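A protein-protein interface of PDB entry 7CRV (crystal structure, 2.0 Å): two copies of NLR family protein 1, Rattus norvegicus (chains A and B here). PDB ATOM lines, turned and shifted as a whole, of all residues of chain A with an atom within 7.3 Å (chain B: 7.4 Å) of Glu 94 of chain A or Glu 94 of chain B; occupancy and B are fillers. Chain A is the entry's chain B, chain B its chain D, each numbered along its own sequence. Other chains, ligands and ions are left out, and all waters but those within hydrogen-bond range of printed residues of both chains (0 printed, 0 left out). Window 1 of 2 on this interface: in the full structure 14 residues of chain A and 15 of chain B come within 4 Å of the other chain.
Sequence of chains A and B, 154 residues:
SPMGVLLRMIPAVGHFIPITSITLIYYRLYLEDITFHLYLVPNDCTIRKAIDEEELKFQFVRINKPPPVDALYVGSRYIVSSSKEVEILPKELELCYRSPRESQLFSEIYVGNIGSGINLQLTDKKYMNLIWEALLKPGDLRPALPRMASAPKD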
ATOM      1  N   PHE A  16      19.998 -16.709 -27.978  1.00  0.00           N
ATOM      2  CA  PHE A  16      20.313 -17.207 -26.641  1.00  0.00           C
ATOM      3  C   PHE A  16      19.080 -17.021 -25.748  1.00  0.00           C
ATOM      4  O   PHE A  16      19.030 -16.156 -24.878  1.00  0.00           O
ATOM      5  CB  PHE A  16      21.585 -16.511 -26.126  1.00  0.00           C
ATOM      6  CG  PHE A  16      22.785 -16.648 -27.068  1.00  0.00           C
ATOM      7  CD1 PHE A  16      23.290 -17.908 -27.403  1.00  0.00           C
ATOM      8  CD2 PHE A  16      23.384 -15.526 -27.642  1.00  0.00           C
ATOM      9  CE1 PHE A  16      24.384 -18.058 -28.273  1.00  0.00           C
ATOM     10  CE2 PHE A  16      24.490 -15.666 -28.527  1.00  0.00           C
ATOM     11  CZ  PHE A  16      24.986 -16.934 -28.836  1.00  0.00           C
ATOM     12  N   LEU A  40      24.255 -32.524 -23.551  1.00  0.00           N
ATOM     13  CA  LEU A  40      23.250 -31.565 -23.102  1.00  0.00           C
ATOM     14  C   LEU A  40      22.749 -30.872 -24.354  1.00  0.00           C
ATOM     15  O   LEU A  40      23.505 -30.151 -25.009  1.00  0.00           O
ATOM     16  CB  LEU A  40      23.823 -30.564 -22.096  1.00  0.00           C
ATOM     17  CG  LEU A  40      22.838 -29.481 -21.600  1.00  0.00           C
ATOM     18  CD1 LEU A  40      21.672 -30.081 -20.837  1.00  0.00           C
ATOM     19  CD2 LEU A  40      23.556 -28.457 -20.730  1.00  0.00           C
ATOM     20  N   VAL A  41      21.494 -31.118 -24.716  1.00  0.00           N
ATOM     21  CA  VAL A  41      20.979 -30.688 -26.014  1.00  0.00           C
ATOM     22  C   VAL A  41      19.543 -30.218 -25.849  1.00  0.00           C
ATOM     23  O   VAL A  41      18.884 -30.512 -24.840  1.00  0.00           O
ATOM     24  CB  VAL A  41      21.044 -31.819 -27.064  1.00  0.00           C
ATOM     25  CG1 VAL A  41      22.500 -32.216 -27.338  1.00  0.00           C
ATOM     26  CG2 VAL A  41      20.224 -33.005 -26.618  1.00  0.00           C
ATOM     27  N   TYR A  73      19.286 -21.539 -20.839  1.00  0.00           N
ATOM     28  CA  TYR A  73      19.416 -20.547 -21.894  1.00  0.00           C
ATOM     29  C   TYR A  73      20.383 -21.065 -22.950  1.00  0.00           C
ATOM     30  O   TYR A  73      21.422 -21.636 -22.621  1.00  0.00           O
ATOM     31  CB  TYR A  73      19.885 -19.201 -21.316  1.00  0.00           C
ATOM     32  CG  TYR A  73      18.718 -18.398 -20.783  1.00  0.00           C
ATOM     33  CD1 TYR A  73      18.269 -18.570 -19.479  1.00  0.00           C
ATOM     34  CD2 TYR A  73      18.028 -17.505 -21.598  1.00  0.00           C
ATOM     35  CE1 TYR A  73      17.165 -17.863 -18.993  1.00  0.00           C
ATOM     36  CE2 TYR A  73      16.925 -16.788 -21.120  1.00  0.00           C
ATOM     37  CZ  TYR A  73      16.497 -16.968 -19.814  1.00  0.00           C
ATOM     38  OH  TYR A  73      15.399 -16.263 -19.330  1.00  0.00           O
ATOM     39  N   VAL A  74      20.005 -20.919 -24.222  1.00  0.00           N
ATOM     40  CA  VAL A  74      20.922 -21.291 -25.289  1.00  0.00           C
ATOM     41  C   VAL A  74      22.215 -20.510 -25.119  1.00  0.00           C
ATOM     42  O   VAL A  74      22.205 -19.325 -24.777  1.00  0.00           O
ATOM     43  CB  VAL A  74      20.282 -21.045 -26.666  1.00  0.00           C
ATOM     44  CG1 VAL A  74      21.316 -21.163 -27.781  1.00  0.00           C
ATOM     45  CG2 VAL A  74      19.163 -22.046 -26.880  1.00  0.00           C
ATOM     46  N   GLY A  75      23.334 -21.186 -25.309  1.00  0.00           N
ATOM     47  CA  GLY A  75      24.627 -20.575 -25.137  1.00  0.00           C
ATOM     48  C   GLY A  75      25.164 -20.592 -23.726  1.00  0.00           C
ATOM     49  O   GLY A  75      26.357 -20.328 -23.543  1.00  0.00           O
ATOM     50  N   SER A  76      24.341 -20.882 -22.714  1.00  0.00           N
ATOM     51  CA  SER A  76      24.896 -20.974 -21.367  1.00  0.00           C
ATOM     52  C   SER A  76      25.861 -22.153 -21.301  1.00  0.00           C
ATOM     53  O   SER A  76      25.795 -23.090 -22.106  1.00  0.00           O
ATOM     54  CB  SER A  76      23.784 -21.069 -20.301  1.00  0.00           C
ATOM     55  OG  SER A  76      22.793 -22.047 -20.591  1.00  0.00           O
ATOM     56  N   ARG A  77      26.824 -22.057 -20.379  1.00  0.00           N
ATOM     57  CA  ARG A  77      27.903 -23.023 -20.235  1.00  0.00           C
ATOM     58  C   ARG A  77      27.841 -23.692 -18.870  1.00  0.00           C
ATOM     59  O   ARG A  77      27.461 -23.071 -17.872  1.00  0.00           O
ATOM     60  CB  ARG A  77      29.256 -22.353 -20.439  1.00  0.00           C
ATOM     61  CG  ARG A  77      29.241 -21.578 -21.739  1.00  0.00           C
ATOM     62  CD  ARG A  77      30.552 -21.607 -22.506  1.00  0.00           C
ATOM     63  NE  ARG A  77      30.287 -21.121 -23.861  1.00  0.00           N
ATOM     64  CZ  ARG A  77      30.722 -19.967 -24.357  1.00  0.00           C
ATOM     65  NH1 ARG A  77      31.481 -19.154 -23.627  1.00  0.00           N
ATOM     66  NH2 ARG A  77      30.403 -19.629 -25.599  1.00  0.00           N
ATOM     67  N   TYR A  78      28.204 -24.975 -18.849  1.00  0.00           N
ATOM     68  CA  TYR A  78      28.056 -25.832 -17.678  1.00  0.00           C
ATOM     69  C   TYR A  78      29.343 -26.600 -17.490  1.00  0.00           C
ATOM     70  O   TYR A  78      30.000 -26.945 -18.469  1.00  0.00           O
ATOM     71  CB  TYR A  78      26.841 -26.790 -17.845  1.00  0.00           C
ATOM     72  CG  TYR A  78      25.592 -25.964 -18.015  1.00  0.00           C
ATOM     73  CD1 TYR A  78      24.957 -25.409 -16.912  1.00  0.00           C
ATOM     74  CD2 TYR A  78      25.121 -25.630 -19.284  1.00  0.00           C
ATOM     75  CE1 TYR A  78      23.863 -24.591 -17.059  1.00  0.00           C
ATOM     76  CE2 TYR A  78      24.017 -24.819 -19.439  1.00  0.00           C
ATOM     77  CZ  TYR A  78      23.395 -24.307 -18.312  1.00  0.00           C
ATOM     78  OH  TYR A  78      22.310 -23.495 -18.445  1.00  0.00           O
ATOM     79  N   GLU A  92      33.729 -28.786 -19.919  1.00  0.00           N
ATOM     80  CA  GLU A  92      32.759 -27.721 -20.081  1.00  0.00           C
ATOM     81  C   GLU A  92      31.883 -27.980 -21.301  1.00  0.00           C
ATOM     82  O   GLU A  92      32.384 -28.280 -22.391  1.00  0.00           O
ATOM     83  CB  GLU A  92      33.498 -26.379 -20.175  1.00  0.00           C
ATOM     84  CG  GLU A  92      32.643 -25.150 -20.005  1.00  0.00           C
ATOM     85  CD  GLU A  92      33.481 -23.870 -20.038  1.00  0.00           C
ATOM     86  OE1 GLU A  92      34.469 -23.785 -19.259  1.00  0.00           O
ATOM     87  OE2 GLU A  92      33.163 -22.972 -20.864  1.00  0.00           O
ATOM     88  N   LEU A  93      30.569 -27.912 -21.100  1.00  0.00           N
ATOM     89  CA  LEU A  93      29.612 -28.077 -22.180  1.00  0.00           C
ATOM     90  C   LEU A  93      28.876 -26.771 -22.403  1.00  0.00           C
ATOM     91  O   LEU A  93      28.610 -26.016 -21.465  1.00  0.00           O
ATOM     92  CB  LEU A  93      28.592 -29.182 -21.887  1.00  0.00           C
ATOM     93  CG  LEU A  93      29.063 -30.628 -21.712  1.00  0.00           C
ATOM     94  CD1 LEU A  93      27.893 -31.501 -21.238  1.00  0.00           C
ATOM     95  CD2 LEU A  93      29.664 -31.160 -23.017  1.00  0.00           C
ATOM     96  N   GLU A  94      28.545 -26.516 -23.654  1.00  0.00           N
ATOM     97  CA  GLU A  94      27.703 -25.397 -24.020  1.00  0.00           C
ATOM     98  C   GLU A  94      26.382 -25.918 -24.565  1.00  0.00           C
ATOM     99  O   GLU A  94      26.356 -26.869 -25.357  1.00  0.00           O
ATOM    100  CB  GLU A  94      28.380 -24.513 -25.063  1.00  0.00           C
ATOM    101  CG  GLU A  94      27.554 -23.282 -25.339  1.00  0.00           C
ATOM    102  CD  GLU A  94      28.192 -22.325 -26.308  1.00  0.00           C
ATOM    103  OE1 GLU A  94      29.439 -22.331 -26.447  1.00  0.00           O
ATOM    104  OE2 GLU A  94      27.425 -21.559 -26.921  1.00  0.00           O
ATOM    105  N   LEU A  95      25.286 -25.297 -24.143  1.00  0.00           N
ATOM    106  CA  LEU A  95      23.966 -25.665 -24.635  1.00  0.00           C
ATOM    107  C   LEU A  95      23.707 -24.905 -25.936  1.00  0.00           C
ATOM    108  O   LEU A  95      23.548 -23.680 -25.931  1.00  0.00           O
ATOM    109  CB  LEU A  95      22.894 -25.367 -23.596  1.00  0.00           C
ATOM    110  CG  LEU A  95      21.463 -25.659 -24.043  1.00  0.00           C
ATOM    111  CD1 LEU A  95      21.299 -27.118 -24.468  1.00  0.00           C
ATOM    112  CD2 LEU A  95      20.480 -25.332 -22.949  1.00  0.00           C
ATOM    113  N   CYS A  96      23.652 -25.627 -27.051  1.00  0.00           N
ATOM    114  CA  CYS A  96      23.314 -24.986 -28.315  1.00  0.00           C
ATOM    115  C   CYS A  96      22.570 -25.974 -29.203  1.00  0.00           C
ATOM    116  O   CYS A  96      22.612 -27.189 -28.995  1.00  0.00           O
ATOM    117  CB  CYS A  96      24.565 -24.482 -29.035  1.00  0.00           C
ATOM    118  SG  CYS A  96      25.806 -25.763 -29.107  1.00  0.00           S
ATOM    119  N   TYR A  97      21.903 -25.435 -30.212  1.00  0.00           N
ATOM    120  CA  TYR A  97      21.253 -26.254 -31.218  1.00  0.00           C
ATOM    121  C   TYR A  97      22.252 -26.554 -32.326  1.00  0.00           C
ATOM    122  O   TYR A  97      22.792 -25.629 -32.942  1.00  0.00           O
ATOM    123  CB  TYR A  97      20.024 -25.554 -31.794  1.00  0.00           C
ATOM    124  CG  TYR A  97      19.405 -26.379 -32.894  1.00  0.00           C
ATOM    125  CD1 TYR A  97      19.788 -26.204 -34.222  1.00  0.00           C
ATOM    126  CD2 TYR A  97      18.479 -27.369 -32.600  1.00  0.00           C
ATOM    127  CE1 TYR A  97      19.243 -26.974 -35.236  1.00  0.00           C
ATOM    128  CE2 TYR A  97      17.923 -28.152 -33.606  1.00  0.00           C
ATOM    129  CZ  TYR A  97      18.311 -27.946 -34.919  1.00  0.00           C
ATOM    130  OH  TYR A  97      17.768 -28.708 -35.919  1.00  0.00           O
ATOM    131  N   ARG A  98      22.497 -27.837 -32.576  1.00  0.00           N
ATOM    132  CA  ARG A  98      23.234 -28.287 -33.747  1.00  0.00           C
ATOM    133  C   ARG A  98      22.353 -29.273 -34.498  1.00  0.00           C
ATOM    134  O   ARG A  98      21.653 -30.081 -33.881  1.00  0.00           O
ATOM    135  CB  ARG A  98      24.564 -28.907 -33.353  1.00  0.00           C
ATOM    136  CG  ARG A  98      25.507 -27.866 -32.771  1.00  0.00           C
ATOM    137  CD  ARG A  98      26.879 -28.411 -32.341  1.00  0.00           C
ATOM    138  NE  ARG A  98      27.393 -29.496 -33.180  1.00  0.00           N
ATOM    139  CZ  ARG A  98      28.683 -29.831 -33.239  1.00  0.00           C
ATOM    140  NH1 ARG A  98      29.085 -30.825 -34.027  1.00  0.00           N
ATOM    141  NH2 ARG A  98      29.570 -29.192 -32.491  1.00  0.00           N
ATOM    142  N   LEU A 105      28.122 -32.110 -29.406  1.00  0.00           N
ATOM    143  CA  LEU A 105      29.147 -31.954 -28.386  1.00  0.00           C
ATOM    144  C   LEU A 105      28.845 -32.840 -27.192  1.00  0.00           C
ATOM    145  O   LEU A 105      27.738 -32.820 -26.661  1.00  0.00           O
ATOM    146  CB  LEU A 105      29.228 -30.501 -27.931  1.00  0.00           C
ATOM    147  CG  LEU A 105      29.700 -29.513 -28.977  1.00  0.00           C
ATOM    148  CD1 LEU A 105      29.887 -28.159 -28.306  1.00  0.00           C
ATOM    149  CD2 LEU A 105      30.994 -30.029 -29.632  1.00  0.00           C
ATOM    150  N   PHE B  16      37.939 -24.240 -26.114  1.00  0.00           N
ATOM    151  CA  PHE B  16      37.832 -22.787 -25.989  1.00  0.00           C
ATOM    152  C   PHE B  16      39.241 -22.215 -25.877  1.00  0.00           C
ATOM    153  O   PHE B  16      39.676 -21.782 -24.809  1.00  0.00           O
ATOM    154  CB  PHE B  16      36.949 -22.403 -24.783  1.00  0.00           C
ATOM    155  CG  PHE B  16      35.600 -23.087 -24.758  1.00  0.00           C
ATOM    156  CD1 PHE B  16      34.565 -22.649 -25.581  1.00  0.00           C
ATOM    157  CD2 PHE B  16      35.360 -24.162 -23.905  1.00  0.00           C
ATOM    158  CE1 PHE B  16      33.302 -23.277 -25.570  1.00  0.00           C
ATOM    159  CE2 PHE B  16      34.108 -24.802 -23.887  1.00  0.00           C
ATOM    160  CZ  PHE B  16      33.074 -24.354 -24.721  1.00  0.00           C
ATOM    161  N   LEU B  40      31.903 -13.355 -38.044  1.00  0.00           N
ATOM    162  CA  LEU B  40      33.136 -13.474 -37.268  1.00  0.00           C
ATOM    163  C   LEU B  40      33.508 -14.954 -37.180  1.00  0.00           C
ATOM    164  O   LEU B  40      32.913 -15.698 -36.402  1.00  0.00           O
ATOM    165  CB  LEU B  40      32.976 -12.868 -35.877  1.00  0.00           C
ATOM    166  CG  LEU B  40      34.253 -12.981 -35.033  1.00  0.00           C
ATOM    167  CD1 LEU B  40      35.415 -12.320 -35.743  1.00  0.00           C
ATOM    168  CD2 LEU B  40      34.034 -12.372 -33.663  1.00  0.00           C
ATOM    169  N   VAL B  41      34.495 -15.383 -37.959  1.00  0.00           N
ATOM    170  CA  VAL B  41      34.739 -16.820 -38.125  1.00  0.00           C
ATOM    171  C   VAL B  41      36.243 -17.084 -38.016  1.00  0.00           C
ATOM    172  O   VAL B  41      37.077 -16.168 -38.114  1.00  0.00           O
ATOM    173  CB  VAL B  41      34.170 -17.332 -39.472  1.00  0.00           C
ATOM    174  CG1 VAL B  41      32.616 -17.211 -39.497  1.00  0.00           C
ATOM    175  CG2 VAL B  41      34.776 -16.540 -40.646  1.00  0.00           C
ATOM    176  N   TYR B  73      39.238 -15.823 -28.544  1.00  0.00           N
ATOM    177  CA  TYR B  73      39.059 -17.152 -27.968  1.00  0.00           C
ATOM    178  C   TYR B  73      37.762 -17.797 -28.461  1.00  0.00           C
ATOM    179  O   TYR B  73      36.695 -17.177 -28.411  1.00  0.00           O
ATOM    180  CB  TYR B  73      39.062 -17.056 -26.440  1.00  0.00           C
ATOM    181  CG  TYR B  73      40.445 -16.934 -25.856  1.00  0.00           C
ATOM    182  CD1 TYR B  73      41.121 -15.717 -25.845  1.00  0.00           C
ATOM    183  CD2 TYR B  73      41.087 -18.038 -25.322  1.00  0.00           C
ATOM    184  CE1 TYR B  73      42.402 -15.608 -25.305  1.00  0.00           C
ATOM    185  CE2 TYR B  73      42.358 -17.941 -24.784  1.00  0.00           C
ATOM    186  CZ  TYR B  73      43.013 -16.728 -24.778  1.00  0.00           C
ATOM    187  OH  TYR B  73      44.280 -16.657 -24.244  1.00  0.00           O
ATOM    188  N   VAL B  74      37.856 -19.048 -28.931  1.00  0.00           N
ATOM    189  CA  VAL B  74      36.656 -19.801 -29.293  1.00  0.00           C
ATOM    190  C   VAL B  74      35.693 -19.814 -28.122  1.00  0.00           C
ATOM    191  O   VAL B  74      36.100 -19.915 -26.961  1.00  0.00           O
ATOM    192  CB  VAL B  74      37.008 -21.240 -29.718  1.00  0.00           C
ATOM    193  CG1 VAL B  74      35.736 -22.049 -29.984  1.00  0.00           C
ATOM    194  CG2 VAL B  74      37.898 -21.239 -30.944  1.00  0.00           C
ATOM    195  N   GLY B  75      34.401 -19.710 -28.429  1.00  0.00           N
ATOM    196  CA  GLY B  75      33.366 -19.595 -27.429  1.00  0.00           C
ATOM    197  C   GLY B  75      33.157 -18.206 -26.854  1.00  0.00           C
ATOM    198  O   GLY B  75      32.141 -17.980 -26.193  1.00  0.00           O
ATOM    199  N   SER B  76      34.093 -17.281 -27.039  1.00  0.00           N
ATOM    200  CA  SER B  76      33.879 -15.955 -26.482  1.00  0.00           C
ATOM    201  C   SER B  76      32.838 -15.211 -27.320  1.00  0.00           C
ATOM    202  O   SER B  76      32.509 -15.603 -28.446  1.00  0.00           O
ATOM    203  CB  SER B  76      35.189 -15.175 -26.391  1.00  0.00           C
ATOM    204  OG  SER B  76      35.774 -14.936 -27.674  1.00  0.00           O
ATOM    205  N   ARG B  77      32.272 -14.159 -26.732  1.00  0.00           N
ATOM    206  CA  ARG B  77      31.132 -13.484 -27.338  1.00  0.00           C
ATOM    207  C   ARG B  77      31.403 -12.001 -27.486  1.00  0.00           C
ATOM    208  O   ARG B  77      32.091 -11.384 -26.651  1.00  0.00           O
ATOM    209  CB  ARG B  77      29.859 -13.679 -26.525  1.00  0.00           C
ATOM    210  CG  ARG B  77      29.483 -15.105 -26.450  1.00  0.00           C
ATOM    211  CD  ARG B  77      28.357 -15.161 -25.503  1.00  0.00           C
ATOM    212  NE  ARG B  77      28.120 -16.575 -25.178  1.00  0.00           N
ATOM    213  CZ  ARG B  77      27.052 -17.041 -24.596  1.00  0.00           C
ATOM    214  NH1 ARG B  77      27.028 -18.317 -24.374  1.00  0.00           N
ATOM    215  NH2 ARG B  77      25.945 -16.295 -24.421  1.00  0.00           N
ATOM    216  N   TYR B  78      30.807 -11.449 -28.530  1.00  0.00           N
ATOM    217  CA  TYR B  78      31.116 -10.123 -29.038  1.00  0.00           C
ATOM    218  C   TYR B  78      29.810  -9.409 -29.332  1.00  0.00           C
ATOM    219  O   TYR B  78      28.891  -9.997 -29.903  1.00  0.00           O
ATOM    220  CB  TYR B  78      32.017 -10.227 -30.289  1.00  0.00           C
ATOM    221  CG  TYR B  78      33.298 -10.902 -29.892  1.00  0.00           C
ATOM    222  CD1 TYR B  78      34.300 -10.180 -29.253  1.00  0.00           C
ATOM    223  CD2 TYR B  78      33.458 -12.268 -30.024  1.00  0.00           C
ATOM    224  CE1 TYR B  78      35.448 -10.792 -28.806  1.00  0.00           C
ATOM    225  CE2 TYR B  78      34.607 -12.890 -29.588  1.00  0.00           C
ATOM    226  CZ  TYR B  78      35.603 -12.137 -28.982  1.00  0.00           C
ATOM    227  OH  TYR B  78      36.758 -12.727 -28.538  1.00  0.00           O
ATOM    228  N   GLU B  92      24.568 -10.097 -30.501  1.00  0.00           N
ATOM    229  CA  GLU B  92      25.658 -10.937 -30.003  1.00  0.00           C
ATOM    230  C   GLU B  92      26.103 -11.926 -31.067  1.00  0.00           C
ATOM    231  O   GLU B  92      25.276 -12.600 -31.688  1.00  0.00           O
ATOM    232  CB  GLU B  92      25.278 -11.726 -28.749  1.00  0.00           C
ATOM    233  CG  GLU B  92      25.215 -10.906 -27.479  1.00  0.00           C
ATOM    234  CD  GLU B  92      25.136 -11.744 -26.182  1.00  0.00           C
ATOM    235  OE1 GLU B  92      25.594 -12.923 -26.151  1.00  0.00           O
ATOM    236  OE2 GLU B  92      24.628 -11.190 -25.178  1.00  0.00           O
ATOM    237  N   LEU B  93      27.410 -12.014 -31.265  1.00  0.00           N
ATOM    238  CA  LEU B  93      28.027 -13.050 -32.077  1.00  0.00           C
ATOM    239  C   LEU B  93      28.930 -13.863 -31.171  1.00  0.00           C
ATOM    240  O   LEU B  93      29.592 -13.311 -30.287  1.00  0.00           O
ATOM    241  CB  LEU B  93      28.865 -12.474 -33.220  1.00  0.00           C
ATOM    242  CG  LEU B  93      28.212 -11.808 -34.430  1.00  0.00           C
ATOM    243  CD1 LEU B  93      29.335 -11.380 -35.390  1.00  0.00           C
ATOM    244  CD2 LEU B  93      27.242 -12.751 -35.109  1.00  0.00           C
ATOM    245  N   GLU B  94      28.963 -15.168 -31.392  1.00  0.00           N
ATOM    246  CA  GLU B  94      29.832 -16.063 -30.645  1.00  0.00           C
ATOM    247  C   GLU B  94      30.847 -16.651 -31.605  1.00  0.00           C
ATOM    248  O   GLU B  94      30.468 -17.181 -32.651  1.00  0.00           O
ATOM    249  CB  GLU B  94      29.022 -17.172 -29.986  1.00  0.00           C
ATOM    250  CG  GLU B  94      29.828 -17.996 -29.035  1.00  0.00           C
ATOM    251  CD  GLU B  94      28.936 -18.857 -28.181  1.00  0.00           C
ATOM    252  OE1 GLU B  94      28.487 -18.393 -27.100  1.00  0.00           O
ATOM    253  OE2 GLU B  94      28.679 -19.996 -28.614  1.00  0.00           O
ATOM    254  N   LEU B  95      32.128 -16.547 -31.271  1.00  0.00           N
ATOM    255  CA  LEU B  95      33.158 -17.061 -32.161  1.00  0.00           C
ATOM    256  C   LEU B  95      33.229 -18.572 -31.992  1.00  0.00           C
ATOM    257  O   LEU B  95      33.406 -19.070 -30.874  1.00  0.00           O
ATOM    258  CB  LEU B  95      34.502 -16.403 -31.861  1.00  0.00           C
ATOM    259  CG  LEU B  95      35.747 -16.961 -32.551  1.00  0.00           C
ATOM    260  CD1 LEU B  95      35.616 -16.867 -34.078  1.00  0.00           C
ATOM    261  CD2 LEU B  95      36.967 -16.192 -32.080  1.00  0.00           C
ATOM    262  N   CYS B  96      33.058 -19.303 -33.087  1.00  0.00           N
ATOM    263  CA  CYS B  96      33.170 -20.751 -33.008  1.00  0.00           C
ATOM    264  C   CYS B  96      33.467 -21.292 -34.396  1.00  0.00           C
ATOM    265  O   CYS B  96      33.270 -20.610 -35.406  1.00  0.00           O
ATOM    266  CB  CYS B  96      31.898 -21.391 -32.441  1.00  0.00           C
ATOM    267  SG  CYS B  96      30.455 -21.088 -33.434  1.00  0.00           S
ATOM    268  N   TYR B  97      33.957 -22.524 -34.425  1.00  0.00           N
ATOM    269  CA  TYR B  97      34.140 -23.241 -35.675  1.00  0.00           C
ATOM    270  C   TYR B  97      32.837 -23.947 -36.025  1.00  0.00           C
ATOM    271  O   TYR B  97      32.294 -24.704 -35.211  1.00  0.00           O
ATOM    272  CB  TYR B  97      35.279 -24.252 -35.563  1.00  0.00           C
ATOM    273  CG  TYR B  97      35.450 -25.070 -36.818  1.00  0.00           C
ATOM    274  CD1 TYR B  97      34.779 -26.284 -36.978  1.00  0.00           C
ATOM    275  CD2 TYR B  97      36.238 -24.610 -37.866  1.00  0.00           C
ATOM    276  CE1 TYR B  97      34.911 -27.029 -38.137  1.00  0.00           C
ATOM    277  CE2 TYR B  97      36.376 -25.344 -39.033  1.00  0.00           C
ATOM    278  CZ  TYR B  97      35.703 -26.554 -39.164  1.00  0.00           C
ATOM    279  OH  TYR B  97      35.828 -27.289 -40.319  1.00  0.00           O
ATOM    280  N   ARG B  98      32.322 -23.689 -37.220  1.00  0.00           N
ATOM    281  CA  ARG B  98      31.271 -24.531 -37.771  1.00  0.00           C
ATOM    282  C   ARG B  98      31.727 -24.961 -39.150  1.00  0.00           C
ATOM    283  O   ARG B  98      32.248 -24.143 -39.915  1.00  0.00           O
ATOM    284  CB  ARG B  98      29.917 -23.815 -37.829  1.00  0.00           C
ATOM    285  CG  ARG B  98      29.460 -23.252 -36.489  1.00  0.00           C
ATOM    286  CD  ARG B  98      28.372 -22.184 -36.667  1.00  0.00           C
ATOM    287  NE  ARG B  98      27.244 -22.722 -37.419  1.00  0.00           N
ATOM    288  CZ  ARG B  98      26.109 -23.134 -36.862  1.00  0.00           C
ATOM    289  NH1 ARG B  98      25.131 -23.634 -37.620  1.00  0.00           N
ATOM    290  NH2 ARG B  98      25.954 -23.034 -35.543  1.00  0.00           N
ATOM    291  N   LEU B 105      26.809 -18.245 -38.865  1.00  0.00           N
ATOM    292  CA  LEU B 105      26.001 -17.182 -38.285  1.00  0.00           C
ATOM    293  C   LEU B 105      26.635 -15.822 -38.533  1.00  0.00           C
ATOM    294  O   LEU B 105      27.862 -15.670 -38.539  1.00  0.00           O
ATOM    295  CB  LEU B 105      25.752 -17.386 -36.789  1.00  0.00           C
ATOM    296  CG  LEU B 105      24.949 -18.667 -36.538  1.00  0.00           C
ATOM    297  CD1 LEU B 105      24.591 -18.856 -35.036  1.00  0.00           C
ATOM    298  CD2 LEU B 105      23.752 -18.857 -37.506  1.00  0.00           C
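Gly 75 of chain A touches Arg 77 of chain B, and with the chains exchanged Arg 77 of chain A touches Gly 75 of chain B. Arg 77 of chain B touches its own counterpart, Arg 77 of chain A. Arg 77 of chain A touches Glu 94 of chain B, but with the chains exchanged Glu 94 of chain A does not touch Arg 77 of chain B (4.1 Å). Glu 94 of chain A touches its own counterpart, Glu 94 of chain B. 17 positions are printed for both chains. Of the 7 pairs that touch across the chains among the printed residues, 6 have their exchanged pair printed and touching as well.
Among the printed residues, pairs that only touch across the chains: Phe 16 of chain A with Glu 92 of chain B, Arg 77 of chain A with Arg 77 of chain B and Glu 92 of chain A with Phe 16 of chain B.
Glu 94 of chain A touches one residue of chain B. Of the printed residues of chain A, Glu 94 of chain B touches Arg 77 (2.7 Å) and Glu 94 (2.6 Å). Of the printed residues of chain B, Gly 75 of chain A touches Arg 77. Printed residues of chain A within 4 Å of Gly 75 of chain B: Arg 77. Of the printed residues of chain A, Glu 92 of chain B touches Phe 16 (3.7 Å). Printed residues of chain B within 4 Å of Phe 16 of chain A: Glu 92 (3.7 Å).
Printed residues of chain A that touch a printed residue of chain B: Phe 16, Gly 75, Arg 77, Glu 92 and Glu 94. Hydrophobic or aromatic side chains of chain B within 4 Å of the printed part of chain A: Phe 16. Along chain B the printed residues that touch a printed residue of chain A span positions 16 to 94. Among the printed residues, 7 pairs touch across the chains.
NH2 of Arg 77 of chain A lies within hydrogen-bond range of O of Gly 75 of chain B (2.5 Å). OE1 of Glu 94 of chain B is in salt-bridge range of NH2 of Arg 77 of chain A (2.7 Å). OE2 of Glu 94 of chain B lies close to OE2 of Glu 94 of chain A, 2.6 Å away. The backbone carbonyl oxygen (O) of Gly 75 of chain A lies close to the guanidinium group (NH1) of Arg 77 of chain B (2.3 Å).
N of Gly 75 of chain B lies within hydrogen-bond range of O of Leu 95 of chain B, 2.7 Å away. The guanidinium group (NH2) of Arg 77 of chain B is in salt-bridge range of the side-chain carboxylate (OE1) of Glu 92 of chain B (3.8 Å). The guanidinium group of Arg 77 of chain B lies within salt-bridge range of the side-chain carboxylate of Glu 94 of chain B. The backbone carbonyl oxygen (O) of Leu 95 of chain A sits at hydrogen-bond distance from the backbone NH (N) of Gly 75 of chain A (2.6 Å). The guanidinium group (NE) of Arg 77 of chain A is in salt-bridge range of the side-chain carboxylate (OE1) of Glu 94 of chain A.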
